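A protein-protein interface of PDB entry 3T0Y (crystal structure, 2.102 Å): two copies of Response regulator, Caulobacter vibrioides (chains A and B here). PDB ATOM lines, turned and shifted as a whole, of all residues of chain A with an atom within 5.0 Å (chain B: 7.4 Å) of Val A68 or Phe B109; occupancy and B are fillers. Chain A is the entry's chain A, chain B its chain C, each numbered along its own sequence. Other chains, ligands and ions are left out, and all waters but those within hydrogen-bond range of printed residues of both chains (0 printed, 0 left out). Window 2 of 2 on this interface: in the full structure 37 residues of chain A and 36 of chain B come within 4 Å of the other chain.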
ATOM      1  N   LEU A  64      -6.130 -17.322   0.979  1.00  0.00           N
ATOM      2  CA  LEU A  64      -7.585 -17.289   0.898  1.00  0.00           C
ATOM      3  C   LEU A  64      -8.113 -15.943   1.391  1.00  0.00           C
ATOM      4  O   LEU A  64      -7.524 -15.354   2.284  1.00  0.00           O
ATOM      5  CB  LEU A  64      -8.164 -18.397   1.787  1.00  0.00           C
ATOM      6  CG  LEU A  64      -7.576 -19.809   1.654  1.00  0.00           C
ATOM      7  CD1 LEU A  64      -8.180 -20.756   2.692  1.00  0.00           C
ATOM      8  CD2 LEU A  64      -7.783 -20.377   0.251  1.00  0.00           C
ATOM      9  N   SER A  65      -9.207 -15.450   0.815  1.00  0.00           N
ATOM     10  CA  SER A  65      -9.851 -14.265   1.366  1.00  0.00           C
ATOM     11  C   SER A  65     -10.119 -14.536   2.836  1.00  0.00           C
ATOM     12  O   SER A  65     -10.145 -15.701   3.262  1.00  0.00           O
ATOM     13  CB  SER A  65     -11.175 -13.992   0.670  1.00  0.00           C
ATOM     14  OG  SER A  65     -12.125 -14.949   1.096  1.00  0.00           O
ATOM     15  N   PRO A  66     -10.310 -13.468   3.627  1.00  0.00           N
ATOM     16  CA  PRO A  66     -10.614 -13.674   5.044  1.00  0.00           C
ATOM     17  C   PRO A  66     -11.893 -14.495   5.243  1.00  0.00           C
ATOM     18  O   PRO A  66     -11.978 -15.296   6.177  1.00  0.00           O
ATOM     19  CB  PRO A  66     -10.791 -12.247   5.572  1.00  0.00           C
ATOM     20  CG  PRO A  66      -9.944 -11.399   4.656  1.00  0.00           C
ATOM     21  CD  PRO A  66     -10.063 -12.043   3.305  1.00  0.00           C
ATOM     22  N   ARG A  67     -12.880 -14.311   4.376  1.00  0.00           N
ATOM     23  CA  ARG A  67     -14.116 -15.066   4.529  1.00  0.00           C
ATOM     24  C   ARG A  67     -13.862 -16.562   4.328  1.00  0.00           C
ATOM     25  O   ARG A  67     -14.107 -17.364   5.205  1.00  0.00           O
ATOM     26  CB  ARG A  67     -15.172 -14.563   3.567  1.00  0.00           C
ATOM     27  CG  ARG A  67     -16.439 -15.360   3.658  1.00  0.00           C
ATOM     28  CD  ARG A  67     -17.535 -14.697   2.877  1.00  0.00           C
ATOM     29  NE  ARG A  67     -18.822 -15.195   3.342  1.00  0.00           N
ATOM     30  CZ  ARG A  67     -19.655 -15.895   2.586  1.00  0.00           C
ATOM     31  NH1 ARG A  67     -19.325 -16.156   1.314  1.00  0.00           N
ATOM     32  NH2 ARG A  67     -20.814 -16.321   3.097  1.00  0.00           N
ATOM     33  N   VAL A  68     -13.331 -16.930   3.175  1.00  0.00           N
ATOM     34  CA  VAL A  68     -12.970 -18.321   2.933  1.00  0.00           C
ATOM     35  C   VAL A  68     -12.078 -18.893   4.037  1.00  0.00           C
ATOM     36  O   VAL A  68     -12.317 -20.006   4.519  1.00  0.00           O
ATOM     37  CB  VAL A  68     -12.286 -18.492   1.578  1.00  0.00           C
ATOM     38  CG1 VAL A  68     -11.732 -19.918   1.430  1.00  0.00           C
ATOM     39  CG2 VAL A  68     -13.267 -18.139   0.455  1.00  0.00           C
ATOM     40  N   ALA A  69     -11.075 -18.124   4.450  1.00  0.00           N
ATOM     41  CA  ALA A  69     -10.124 -18.577   5.463  1.00  0.00           C
ATOM     42  C   ALA A  69     -10.796 -18.831   6.805  1.00  0.00           C
ATOM     43  O   ALA A  69     -10.379 -19.707   7.549  1.00  0.00           O
ATOM     44  CB  ALA A  69      -8.992 -17.552   5.635  1.00  0.00           C
ATOM     45  N   LEU A  70     -11.810 -18.033   7.129  1.00  0.00           N
ATOM     46  CA  LEU A  70     -12.531 -18.201   8.383  1.00  0.00           C
ATOM     47  C   LEU A  70     -13.271 -19.540   8.369  1.00  0.00           C
ATOM     48  O   LEU A  70     -13.171 -20.331   9.312  1.00  0.00           O
ATOM     49  CB  LEU A  70     -13.542 -17.071   8.596  1.00  0.00           C
ATOM     50  CG  LEU A  70     -14.446 -17.241   9.816  1.00  0.00           C
ATOM     51  CD1 LEU A  70     -13.599 -17.137  11.101  1.00  0.00           C
ATOM     52  CD2 LEU A  70     -15.597 -16.200   9.837  1.00  0.00           C
ATOM     53  N   TYR A  71     -14.031 -19.786   7.307  1.00  0.00           N
ATOM     54  CA  TYR A  71     -14.706 -21.067   7.198  1.00  0.00           C
ATOM     55  C   TYR A  71     -13.716 -22.233   7.148  1.00  0.00           C
ATOM     56  O   TYR A  71     -14.019 -23.297   7.651  1.00  0.00           O
ATOM     57  CB  TYR A  71     -15.609 -21.109   5.983  1.00  0.00           C
ATOM     58  CG  TYR A  71     -16.865 -20.280   6.096  1.00  0.00           C
ATOM     59  CD1 TYR A  71     -16.807 -18.909   6.107  1.00  0.00           C
ATOM     60  CD2 TYR A  71     -18.117 -20.879   6.154  1.00  0.00           C
ATOM     61  CE1 TYR A  71     -17.944 -18.147   6.181  1.00  0.00           C
ATOM     62  CE2 TYR A  71     -19.272 -20.115   6.221  1.00  0.00           C
ATOM     63  CZ  TYR A  71     -19.171 -18.746   6.234  1.00  0.00           C
ATOM     64  OH  TYR A  71     -20.298 -17.958   6.296  1.00  0.00           O
ATOM     65  N   ARG A  72     -12.544 -22.053   6.547  1.00  0.00           N
ATOM     66  CA  ARG A  72     -11.543 -23.122   6.589  1.00  0.00           C
ATOM     67  C   ARG A  72     -11.150 -23.411   8.031  1.00  0.00           C
ATOM     68  O   ARG A  72     -11.035 -24.565   8.406  1.00  0.00           O
ATOM     69  CB  ARG A  72     -10.299 -22.813   5.750  1.00  0.00           C
ATOM     70  CG  ARG A  72      -9.244 -23.918   5.818  1.00  0.00           C
ATOM     71  CD  ARG A  72      -8.018 -23.571   4.951  1.00  0.00           C
ATOM     72  NE  ARG A  72      -6.911 -24.541   5.027  1.00  0.00           N
ATOM     73  CZ  ARG A  72      -6.674 -25.497   4.126  1.00  0.00           C
ATOM     74  NH1 ARG A  72      -7.466 -25.639   3.068  1.00  0.00           N
ATOM     75  NH2 ARG A  72      -5.646 -26.322   4.283  1.00  0.00           N
ATOM     76  N   ALA B 100     -20.698 -29.643   2.362  1.00  0.00           N
ATOM     77  CA  ALA B 100     -20.371 -29.327   0.986  1.00  0.00           C
ATOM     78  C   ALA B 100     -21.555 -28.658   0.325  1.00  0.00           C
ATOM     79  O   ALA B 100     -21.407 -27.701  -0.430  1.00  0.00           O
ATOM     80  CB  ALA B 100     -20.023 -30.575   0.258  1.00  0.00           C
ATOM     81  N   PHE B 101     -22.738 -29.174   0.614  1.00  0.00           N
ATOM     82  CA  PHE B 101     -23.951 -28.627   0.056  1.00  0.00           C
ATOM     83  C   PHE B 101     -24.225 -27.214   0.588  1.00  0.00           C
ATOM     84  O   PHE B 101     -24.529 -26.310  -0.186  1.00  0.00           O
ATOM     85  CB  PHE B 101     -25.134 -29.547   0.372  1.00  0.00           C
ATOM     86  CG  PHE B 101     -26.448 -29.030  -0.130  1.00  0.00           C
ATOM     87  CD1 PHE B 101     -26.765 -29.099  -1.484  1.00  0.00           C
ATOM     88  CD2 PHE B 101     -27.373 -28.482   0.743  1.00  0.00           C
ATOM     89  CE1 PHE B 101     -27.996 -28.633  -1.959  1.00  0.00           C
ATOM     90  CE2 PHE B 101     -28.604 -28.008   0.273  1.00  0.00           C
ATOM     91  CZ  PHE B 101     -28.910 -28.082  -1.078  1.00  0.00           C
ATOM     92  N   LEU B 102     -24.122 -27.017   1.900  1.00  0.00           N
ATOM     93  CA  LEU B 102     -24.413 -25.710   2.460  1.00  0.00           C
ATOM     94  C   LEU B 102     -23.361 -24.674   2.091  1.00  0.00           C
ATOM     95  O   LEU B 102     -23.689 -23.504   1.920  1.00  0.00           O
ATOM     96  CB  LEU B 102     -24.599 -25.764   3.986  1.00  0.00           C
ATOM     97  CG  LEU B 102     -25.843 -26.510   4.473  1.00  0.00           C
ATOM     98  CD1 LEU B 102     -25.839 -26.548   5.965  1.00  0.00           C
ATOM     99  CD2 LEU B 102     -27.108 -25.843   3.980  1.00  0.00           C
ATOM    100  N   LEU B 103     -22.099 -25.087   1.983  1.00  0.00           N
ATOM    101  CA  LEU B 103     -21.059 -24.137   1.634  1.00  0.00           C
ATOM    102  C   LEU B 103     -21.369 -23.531   0.258  1.00  0.00           C
ATOM    103  O   LEU B 103     -21.166 -22.344   0.038  1.00  0.00           O
ATOM    104  CB  LEU B 103     -19.676 -24.788   1.641  1.00  0.00           C
ATOM    105  CG  LEU B 103     -19.150 -25.050   3.050  1.00  0.00           C
ATOM    106  CD1 LEU B 103     -17.997 -26.040   2.989  1.00  0.00           C
ATOM    107  CD2 LEU B 103     -18.714 -23.737   3.725  1.00  0.00           C
ATOM    108  N   THR B 104     -21.882 -24.348  -0.653  1.00  0.00           N
ATOM    109  CA  THR B 104     -22.145 -23.877  -2.002  1.00  0.00           C
ATOM    110  C   THR B 104     -23.554 -23.284  -2.127  1.00  0.00           C
ATOM    111  O   THR B 104     -23.710 -22.112  -2.460  1.00  0.00           O
ATOM    112  CB  THR B 104     -21.888 -24.993  -3.042  1.00  0.00           C
ATOM    113  OG1 THR B 104     -22.571 -26.198  -2.649  1.00  0.00           O
ATOM    114  CG2 THR B 104     -20.399 -25.300  -3.111  1.00  0.00           C
ATOM    115  N   ALA B 105     -24.577 -24.069  -1.822  1.00  0.00           N
ATOM    116  CA  ALA B 105     -25.952 -23.624  -2.026  1.00  0.00           C
ATOM    117  C   ALA B 105     -26.347 -22.466  -1.128  1.00  0.00           C
ATOM    118  O   ALA B 105     -27.029 -21.541  -1.576  1.00  0.00           O
ATOM    119  CB  ALA B 105     -26.916 -24.774  -1.828  1.00  0.00           C
ATOM    120  N   LEU B 106     -25.946 -22.523   0.141  1.00  0.00           N
ATOM    121  CA  LEU B 106     -26.337 -21.494   1.101  1.00  0.00           C
ATOM    122  C   LEU B 106     -25.326 -20.364   1.244  1.00  0.00           C
ATOM    123  O   LEU B 106     -25.691 -19.186   1.245  1.00  0.00           O
ATOM    124  CB  LEU B 106     -26.599 -22.112   2.477  1.00  0.00           C
ATOM    125  CG  LEU B 106     -26.890 -21.122   3.610  1.00  0.00           C
ATOM    126  CD1 LEU B 106     -28.190 -20.356   3.357  1.00  0.00           C
ATOM    127  CD2 LEU B 106     -26.935 -21.805   4.980  1.00  0.00           C
ATOM    128  N   GLU B 107     -24.056 -20.713   1.407  1.00  0.00           N
ATOM    129  CA  GLU B 107     -23.063 -19.687   1.724  1.00  0.00           C
ATOM    130  C   GLU B 107     -22.438 -19.099   0.459  1.00  0.00           C
ATOM    131  O   GLU B 107     -21.609 -18.195   0.537  1.00  0.00           O
ATOM    132  CB  GLU B 107     -21.975 -20.229   2.648  1.00  0.00           C
ATOM    133  CG  GLU B 107     -22.448 -20.632   4.034  1.00  0.00           C
ATOM    134  CD  GLU B 107     -23.169 -19.507   4.764  1.00  0.00           C
ATOM    135  OE1 GLU B 107     -22.672 -18.356   4.767  1.00  0.00           O
ATOM    136  OE2 GLU B 107     -24.250 -19.784   5.326  1.00  0.00           O
ATOM    137  N   GLY B 108     -22.834 -19.625  -0.696  1.00  0.00           N
ATOM    138  CA  GLY B 108     -22.428 -19.082  -1.986  1.00  0.00           C
ATOM    139  C   GLY B 108     -20.956 -19.188  -2.344  1.00  0.00           C
ATOM    140  O   GLY B 108     -20.482 -18.468  -3.221  1.00  0.00           O
ATOM    141  N   PHE B 109     -20.218 -20.075  -1.683  1.00  0.00           N
ATOM    142  CA  PHE B 109     -18.850 -20.356  -2.109  1.00  0.00           C
ATOM    143  C   PHE B 109     -18.879 -21.177  -3.386  1.00  0.00           C
ATOM    144  O   PHE B 109     -19.820 -21.941  -3.622  1.00  0.00           O
ATOM    145  CB  PHE B 109     -18.092 -21.120  -1.035  1.00  0.00           C
ATOM    146  CG  PHE B 109     -17.890 -20.328   0.211  1.00  0.00           C
ATOM    147  CD1 PHE B 109     -16.936 -19.322   0.250  1.00  0.00           C
ATOM    148  CD2 PHE B 109     -18.682 -20.551   1.323  1.00  0.00           C
ATOM    149  CE1 PHE B 109     -16.749 -18.568   1.393  1.00  0.00           C
ATOM    150  CE2 PHE B 109     -18.494 -19.813   2.474  1.00  0.00           C
ATOM    151  CZ  PHE B 109     -17.524 -18.816   2.507  1.00  0.00           C
ATOM    152  N   THR B 110     -17.850 -21.037  -4.210  1.00  0.00           N
ATOM    153  CA  THR B 110     -17.764 -21.858  -5.408  1.00  0.00           C
ATOM    154  C   THR B 110     -17.296 -23.219  -4.955  1.00  0.00           C
ATOM    155  O   THR B 110     -16.722 -23.342  -3.868  1.00  0.00           O
ATOM    156  CB  THR B 110     -16.781 -21.280  -6.429  1.00  0.00           C
ATOM    157  OG1 THR B 110     -15.462 -21.250  -5.864  1.00  0.00           O
ATOM    158  CG2 THR B 110     -17.187 -19.864  -6.799  1.00  0.00           C
ATOM    159  N   PRO B 111     -17.561 -24.256  -5.764  1.00  0.00           N
ATOM    160  CA  PRO B 111     -17.046 -25.581  -5.433  1.00  0.00           C
ATOM    161  C   PRO B 111     -15.536 -25.577  -5.159  1.00  0.00           C
ATOM    162  O   PRO B 111     -15.087 -26.337  -4.305  1.00  0.00           O
ATOM    163  CB  PRO B 111     -17.390 -26.407  -6.680  1.00  0.00           C
ATOM    164  CG  PRO B 111     -18.624 -25.764  -7.191  1.00  0.00           C
ATOM    165  CD  PRO B 111     -18.460 -24.285  -6.925  1.00  0.00           C
ATOM    166  N   THR B 112     -14.768 -24.761  -5.869  1.00  0.00           N
ATOM    167  CA  THR B 112     -13.315 -24.703  -5.653  1.00  0.00           C
ATOM    168  C   THR B 112     -13.042 -24.157  -4.256  1.00  0.00           C
ATOM    169  O   THR B 112     -12.188 -24.658  -3.524  1.00  0.00           O
ATOM    170  CB  THR B 112     -12.615 -23.758  -6.656  1.00  0.00           C
ATOM    171  OG1 THR B 112     -12.698 -24.297  -7.974  1.00  0.00           O
ATOM    172  CG2 THR B 112     -11.144 -23.548  -6.276  1.00  0.00           C
ATOM    173  N   GLU B 113     -13.761 -23.108  -3.893  1.00  0.00           N
ATOM    174  CA  GLU B 113     -13.554 -22.516  -2.584  1.00  0.00           C
ATOM    175  C   GLU B 113     -13.990 -23.532  -1.520  1.00  0.00           C
ATOM    176  O   GLU B 113     -13.337 -23.681  -0.496  1.00  0.00           O
ATOM    177  CB  GLU B 113     -14.341 -21.210  -2.456  1.00  0.00           C
ATOM    178  CG  GLU B 113     -13.764 -20.074  -3.264  1.00  0.00           C
ATOM    179  CD  GLU B 113     -14.683 -18.865  -3.331  1.00  0.00           C
ATOM    180  OE1 GLU B 113     -15.910 -19.024  -3.202  1.00  0.00           O
ATOM    181  OE2 GLU B 113     -14.177 -17.738  -3.510  1.00  0.00           O
ATOM    182  N   ALA B 114     -15.077 -24.254  -1.776  1.00  0.00           N
ATOM    183  CA  ALA B 114     -15.556 -25.244  -0.803  1.00  0.00           C
ATOM    184  C   ALA B 114     -14.495 -26.332  -0.588  1.00  0.00           C
ATOM    185  O   ALA B 114     -14.326 -26.839   0.511  1.00  0.00           O
ATOM    186  CB  ALA B 114     -16.890 -25.854  -1.246  1.00  0.00           C
ATOM    187  N   ALA B 115     -13.767 -26.655  -1.645  1.00  0.00           N
ATOM    188  CA  ALA B 115     -12.664 -27.607  -1.578  1.00  0.00           C
ATOM    189  C   ALA B 115     -11.576 -27.104  -0.642  1.00  0.00           C
ATOM    190  O   ALA B 115     -11.058 -27.861   0.173  1.00  0.00           O
ATOM    191  CB  ALA B 115     -12.081 -27.856  -2.989  1.00  0.00           C
ATOM    192  N   GLN B 116     -11.222 -25.826  -0.753  1.00  0.00           N
ATOM    193  CA  GLN B 116     -10.236 -25.260   0.166  1.00  0.00           C
ATOM    194  C   GLN B 116     -10.752 -25.334   1.595  1.00  0.00           C
ATOM    195  O   GLN B 116     -10.027 -25.719   2.528  1.00  0.00           O
ATOM    196  CB  GLN B 116      -9.927 -23.814  -0.195  1.00  0.00           C
ATOM    197  CG  GLN B 116      -9.669 -23.611  -1.680  1.00  0.00           C
ATOM    198  CD  GLN B 116      -8.626 -24.579  -2.198  1.00  0.00           C
ATOM    199  OE1 GLN B 116      -7.490 -24.591  -1.713  1.00  0.00           O
ATOM    200  NE2 GLN B 116      -9.015 -25.425  -3.164  1.00  0.00           N
ATOM    201  N   ILE B 117     -12.016 -24.961   1.760  1.00  0.00           N
ATOM    202  CA  ILE B 117     -12.611 -24.910   3.074  1.00  0.00           C
ATOM    203  C   ILE B 117     -12.601 -26.304   3.731  1.00  0.00           C
ATOM    204  O   ILE B 117     -12.228 -26.461   4.891  1.00  0.00           O
ATOM    205  CB  ILE B 117     -14.041 -24.303   3.000  1.00  0.00           C
ATOM    206  CG1 ILE B 117     -13.954 -22.797   2.710  1.00  0.00           C
ATOM    207  CG2 ILE B 117     -14.801 -24.565   4.286  1.00  0.00           C
ATOM    208  CD1 ILE B 117     -15.284 -22.151   2.280  1.00  0.00           C
ATOM    209  N   ILE B 129     -21.565 -33.056  -2.835  1.00  0.00           N
ATOM    210  CA  ILE B 129     -22.743 -32.297  -3.227  1.00  0.00           C
ATOM    211  C   ILE B 129     -23.716 -33.196  -3.985  1.00  0.00           C
ATOM    212  O   ILE B 129     -24.938 -33.027  -3.904  1.00  0.00           O
ATOM    213  CB  ILE B 129     -22.375 -31.139  -4.157  1.00  0.00           C
ATOM    214  CG1 ILE B 129     -21.542 -30.084  -3.419  1.00  0.00           C
ATOM    215  CG2 ILE B 129     -23.637 -30.507  -4.722  1.00  0.00           C
ATOM    216  CD1 ILE B 129     -20.919 -29.050  -4.385  1.00  0.00           C
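Arg A67 touches Phe B109.
CG2 of Val A68 touches CE1 of Phe B109, 3.6 Å away.
O of Val A68 touches CG1 of Ile B117 (3.7 Å).
Tyr A71 touches Leu B103 (CD2 to CD2, 3.8 Å).
Tyr A71 touches Phe B109 (CD1 to CZ, 3.7 Å).
O of Tyr A71 touches CG2 of Ile B117, at 3.7 Å.
Arg A72 touches Ile B117.
OG of Ser A65 lies close to N of Arg A67 (3.4 Å).
The backbone NH (N) of Val A68 is in hydrogen-bond range of the side-chain hydroxyl (OG) of Ser A65, 3.1 Å away.
N of Glu B107 lies within hydrogen-bond range of O of Leu B102.
The backbone carbonyl oxygen (O) of Leu B103 is in hydrogen-bond range of the backbone NH (N) of Gly B108.
N of Phe B109 lies within hydrogen-bond range of O of Leu B103 (3.0 Å).
The side-chain amide nitrogen (NE2) of Gln B116 is in hydrogen-bond range of the backbone carbonyl oxygen (O) of Thr B112 (3.3 Å).
Val A68 touches just these residues of chain B: Phe B109 and Ile B117.
Of chain A, only Arg A67, Val A68 and Tyr A71 come within 4 Å of Phe B109.
Of the printed residues of chain B, Arg A72 touches Gln B116 (2.6 Å) and Ile B117 (3.8 Å).
Of the printed residues of chain A, Ile B117 touches Val A68 (3.7 Å), Tyr A71 (3.7 Å) and Arg A72 (3.8 Å).
Thr B112 touches none of the printed residues of chain A.
Leu B102 touches none of the printed residues of chain A.
The nearest residue of chain B that does not touch Val A68 is Glu B113 (4.1 Å).
The nearest printed residue of chain A that does not touch Phe B109 is Ser A65 (5.9 Å).
The nearest printed residue of chain B that does not touch Tyr A71 is Gln B116 (6.9 Å).
Of the 9 printed residues of chain A, 4 touch a printed residue of chain B.
Hydrophobic or aromatic side chains of chain A within 4 Å of the printed part of chain B: Val A68 and Tyr A71.
Among the printed residues, Asp or Glu carboxylates within 4 Å of a Lys or Arg side-chain nitrogen of the other chain: Arg A67 with Glu B107 (3.2 Å).
NH2 of Arg A67 is in salt-bridge range of OE1 of Glu B107, 3.2 Å away.
The side-chain hydroxyl of Tyr A71 lies within hydrogen-bond range of the side-chain carboxylate of Glu B107.
The guanidinium group of Arg A72 sits at hydrogen-bond distance from the backbone carbonyl oxygen of Gln B116, 2.6 Å away.
No position is printed for both chains.
Of the 10 pairs that touch across the chains among the printed residues, none has its exchanged pair printed and touching as well.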
